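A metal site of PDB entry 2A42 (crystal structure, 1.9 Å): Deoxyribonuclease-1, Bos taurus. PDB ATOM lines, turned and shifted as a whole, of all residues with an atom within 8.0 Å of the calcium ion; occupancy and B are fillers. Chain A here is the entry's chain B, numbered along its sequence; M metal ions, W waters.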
ATOM      1  N   ALA A 200      12.209   0.685  14.240  1.00  0.00           N
ATOM      2  CA  ALA A 200      10.777   0.894  14.026  1.00  0.00           C
ATOM      3  C   ALA A 200      10.191  -0.266  13.256  1.00  0.00           C
ATOM      4  O   ALA A 200      10.862  -0.824  12.391  1.00  0.00           O
ATOM      5  CB  ALA A 200      10.542   2.197  13.225  1.00  0.00           C
ATOM      6  N   ASP A 201       8.910  -0.539  13.495  1.00  0.00           N
ATOM      7  CA  ASP A 201       8.185  -1.573  12.738  1.00  0.00           C
ATOM      8  C   ASP A 201       7.239  -0.869  11.757  1.00  0.00           C
ATOM      9  O   ASP A 201       6.264  -0.216  12.177  1.00  0.00           O
ATOM     10  CB  ASP A 201       7.368  -2.414  13.738  1.00  0.00           C
ATOM     11  CG  ASP A 201       6.439  -3.406  13.052  1.00  0.00           C
ATOM     12  OD1 ASP A 201       6.746  -3.895  11.947  1.00  0.00           O
ATOM     13  OD2 ASP A 201       5.378  -3.714  13.620  1.00  0.00           O
ATOM     14  N   THR A 202       7.508  -0.988  10.456  1.00  0.00           N
ATOM     15  CA  THR A 202       6.668  -0.316   9.460  1.00  0.00           C
ATOM     16  C   THR A 202       5.789  -1.316   8.710  1.00  0.00           C
ATOM     17  O   THR A 202       5.127  -0.949   7.722  1.00  0.00           O
ATOM     18  CB  THR A 202       7.510   0.563   8.490  1.00  0.00           C
ATOM     19  OG1 THR A 202       8.241  -0.277   7.581  1.00  0.00           O
ATOM     20  CG2 THR A 202       8.513   1.414   9.261  1.00  0.00           C
ATOM     21  N   THR A 203       5.753  -2.559   9.175  1.00  0.00           N
ATOM     22  CA  THR A 203       4.853  -3.564   8.577  1.00  0.00           C
ATOM     23  C   THR A 203       3.605  -3.832   9.392  1.00  0.00           C
ATOM     24  O   THR A 203       3.661  -3.925  10.624  1.00  0.00           O
ATOM     25  CB  THR A 203       5.576  -4.883   8.310  1.00  0.00           C
ATOM     26  OG1 THR A 203       5.731  -5.624   9.530  1.00  0.00           O
ATOM     27  CG2 THR A 203       6.930  -4.587   7.686  1.00  0.00           C
ATOM     28  N   ALA A 204       2.463  -3.949   8.704  1.00  0.00           N
ATOM     29  CA  ALA A 204       1.194  -4.257   9.379  1.00  0.00           C
ATOM     30  C   ALA A 204       1.120  -5.747   9.669  1.00  0.00           C
ATOM     31  O   ALA A 204       0.312  -6.175  10.479  1.00  0.00           O
ATOM     32  CB  ALA A 204      -0.002  -3.808   8.532  1.00  0.00           C
ATOM     33  N   THR A 205       2.014  -6.527   9.057  1.00  0.00           N
ATOM     34  CA  THR A 205       2.042  -7.960   9.300  1.00  0.00           C
ATOM     35  C   THR A 205       2.870  -8.226  10.548  1.00  0.00           C
ATOM     36  O   THR A 205       3.423  -7.302  11.118  1.00  0.00           O
ATOM     37  CB  THR A 205       2.768  -8.671   8.156  1.00  0.00           C
ATOM     38  OG1 THR A 205       4.099  -8.169   8.094  1.00  0.00           O
ATOM     39  CG2 THR A 205       2.081  -8.364   6.829  1.00  0.00           C
ATOM     40  N   SER A 206       2.951  -9.494  10.939  1.00  0.00           N
ATOM     41  CA  SER A 206       3.755  -9.924  12.085  1.00  0.00           C
ATOM     42  C   SER A 206       5.278  -9.864  11.997  1.00  0.00           C
ATOM     43  O   SER A 206       5.979 -10.248  12.930  1.00  0.00           O
ATOM     44  CB  SER A 206       3.339 -11.344  12.479  1.00  0.00           C
ATOM     45  OG  SER A 206       3.831 -12.259  11.528  1.00  0.00           O
ATOM     46  N   THR A 207       5.829  -9.401  10.882  1.00  0.00           N
ATOM     47  CA  THR A 207       7.264  -9.169  10.854  1.00  0.00           C
ATOM     48  C   THR A 207       7.578  -7.882  11.594  1.00  0.00           C
ATOM     49  O   THR A 207       6.702  -7.020  11.750  1.00  0.00           O
ATOM     50  CB  THR A 207       7.802  -9.070   9.430  1.00  0.00           C
ATOM     51  OG1 THR A 207       7.181  -7.973   8.741  1.00  0.00           O
ATOM     52  CG2 THR A 207       7.510 -10.365   8.683  1.00  0.00           C
ATOM     53  N   ASN A 208       8.816  -7.747  12.066  1.00  0.00           N
ATOM     54  CA  ASN A 208       9.240  -6.536  12.731  1.00  0.00           C
ATOM     55  C   ASN A 208      10.376  -5.894  11.944  1.00  0.00           C
ATOM     56  O   ASN A 208      11.549  -6.190  12.168  1.00  0.00           O
ATOM     57  CB  ASN A 208       9.649  -6.818  14.171  1.00  0.00           C
ATOM     58  CG  ASN A 208      10.311  -5.635  14.810  1.00  0.00           C
ATOM     59  OD1 ASN A 208       9.916  -4.509  14.535  1.00  0.00           O
ATOM     60  ND2 ASN A 208      11.347  -5.872  15.601  1.00  0.00           N
ATOM     61  N   CYS A 209      10.030  -5.021  10.989  1.00  0.00           N
ATOM     62  CA  CYS A 209      10.992  -4.540  10.005  1.00  0.00           C
ATOM     63  C   CYS A 209      10.790  -3.046   9.747  1.00  0.00           C
ATOM     64  O   CYS A 209       9.659  -2.611   9.571  1.00  0.00           O
ATOM     65  CB  CYS A 209      10.832  -5.283   8.666  1.00  0.00           C
ATOM     66  SG  CYS A 209      11.107  -7.071   8.767  1.00  0.00           S
ATOM     67  N   ASP A 234       0.534   3.424  12.942  1.00  0.00           N
ATOM     68  CA  ASP A 234      -0.073   2.097  13.135  1.00  0.00           C
ATOM     69  C   ASP A 234      -1.601   2.245  13.063  1.00  0.00           C
ATOM     70  O   ASP A 234      -2.262   2.456  14.073  1.00  0.00           O
ATOM     71  CB  ASP A 234       0.395   1.454  14.455  1.00  0.00           C
ATOM     72  CG  ASP A 234      -0.304   0.123  14.761  1.00  0.00           C
ATOM     73  OD1 ASP A 234      -1.270  -0.225  14.043  1.00  0.00           O
ATOM     74  OD2 ASP A 234       0.085  -0.576  15.740  1.00  0.00           O
ATOM     75  N   ASN A 243      -6.675  -7.331  12.910  1.00  0.00           N
ATOM     76  CA  ASN A 243      -5.479  -7.467  12.074  1.00  0.00           C
ATOM     77  C   ASN A 243      -5.849  -7.809  10.637  1.00  0.00           C
ATOM     78  O   ASN A 243      -5.215  -7.335   9.702  1.00  0.00           O
ATOM     79  CB  ASN A 243      -4.477  -8.492  12.629  1.00  0.00           C
ATOM     80  CG  ASN A 243      -3.182  -8.519  11.816  1.00  0.00           C
ATOM     81  OD1 ASN A 243      -2.827  -9.533  11.217  1.00  0.00           O
ATOM     82  ND2 ASN A 243      -2.490  -7.401  11.776  1.00  0.00           N
ATOM     83  N   LEU A 247      -4.729  -5.770   7.414  1.00  0.00           N
ATOM     84  CA  LEU A 247      -3.952  -6.273   6.264  1.00  0.00           C
ATOM     85  C   LEU A 247      -4.678  -6.125   4.936  1.00  0.00           C
ATOM     86  O   LEU A 247      -4.053  -6.049   3.859  1.00  0.00           O
ATOM     87  CB  LEU A 247      -3.590  -7.740   6.449  1.00  0.00           C
ATOM     88  CG  LEU A 247      -2.773  -8.070   7.698  1.00  0.00           C
ATOM     89  CD1 LEU A 247      -2.690  -9.567   7.836  1.00  0.00           C
ATOM     90  CD2 LEU A 247      -1.404  -7.409   7.637  1.00  0.00           C
ATOM     91  N   ASP A 251      -0.141  -4.261   3.753  1.00  0.00           N
ATOM     92  CA  ASP A 251       0.847  -4.927   4.625  1.00  0.00           C
ATOM     93  C   ASP A 251       1.892  -3.983   5.217  1.00  0.00           C
ATOM     94  O   ASP A 251       2.784  -4.420   5.960  1.00  0.00           O
ATOM     95  CB  ASP A 251       1.498  -6.137   3.943  1.00  0.00           C
ATOM     96  CG  ASP A 251       2.143  -5.814   2.611  1.00  0.00           C
ATOM     97  OD1 ASP A 251       1.977  -4.700   2.046  1.00  0.00           O
ATOM     98  OD2 ASP A 251       2.869  -6.720   2.137  1.00  0.00           O
ATOM     99  N   HIS A 252       1.815  -2.698   4.874  1.00  0.00           N
ATOM    100  CA  HIS A 252       2.701  -1.696   5.477  1.00  0.00           C
ATOM    101  C   HIS A 252       1.932  -0.608   6.190  1.00  0.00           C
ATOM    102  O   HIS A 252       0.801  -0.329   5.824  1.00  0.00           O
ATOM    103  CB  HIS A 252       3.489  -0.963   4.390  1.00  0.00           C
ATOM    104  CG  HIS A 252       4.507  -1.815   3.724  1.00  0.00           C
ATOM    105  ND1 HIS A 252       5.859  -1.663   3.942  1.00  0.00           N
ATOM    106  CD2 HIS A 252       4.373  -2.809   2.814  1.00  0.00           C
ATOM    107  CE1 HIS A 252       6.513  -2.547   3.196  1.00  0.00           C
ATOM    108  NE2 HIS A 252       5.631  -3.240   2.497  1.00  0.00           N
ATOM    109  N   TYR A 253       2.572   0.043   7.175  1.00  0.00           N
ATOM    110  CA  TYR A 253       2.092   1.301   7.708  1.00  0.00           C
ATOM    111  C   TYR A 253       2.709   2.448   6.924  1.00  0.00           C
ATOM    112  O   TYR A 253       3.846   2.327   6.447  1.00  0.00           O
ATOM    113  CB  TYR A 253       2.501   1.504   9.194  1.00  0.00           C
ATOM    114  CG  TYR A 253       2.123   0.386  10.111  1.00  0.00           C
ATOM    115  CD1 TYR A 253       0.808  -0.094  10.139  1.00  0.00           C
ATOM    116  CD2 TYR A 253       3.041  -0.147  11.029  1.00  0.00           C
ATOM    117  CE1 TYR A 253       0.447  -1.101  11.007  1.00  0.00           C
ATOM    118  CE2 TYR A 253       2.688  -1.165  11.894  1.00  0.00           C
ATOM    119  CZ  TYR A 253       1.387  -1.630  11.875  1.00  0.00           C
ATOM    120  OH  TYR A 253       1.018  -2.644  12.715  1.00  0.00           O
HETATM  121 CA    CA M   1       4.814  -5.474  12.023  1.00  0.00          CA
HETATM  122  O   HOH W   1       2.753  -5.013  13.144  1.00  0.00           O
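Four residues have an atom within 4 Å of the calcium ion: Asp 201, Thr 203, Thr 205 and Thr 207. The nearest printed residue that does not touch the calcium ion is Ala 204 (4.3 Å).
The side-chain hydroxyl (OG1) of Thr 207 is in hydrogen-bond range of the side-chain hydroxyl (OG1) of Thr 205 (3.2 Å).
The calcium ion is bound by O of Thr 203 (2.4 Å), water W1 (2.4 Å), OD2 of Asp 201 (2.4 Å), O of Thr 207 (2.5 Å), O of Thr 205 (2.5 Å), OD1 of Asp 201 (2.5 Å) and OG1 of Thr 203 (2.7 Å).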
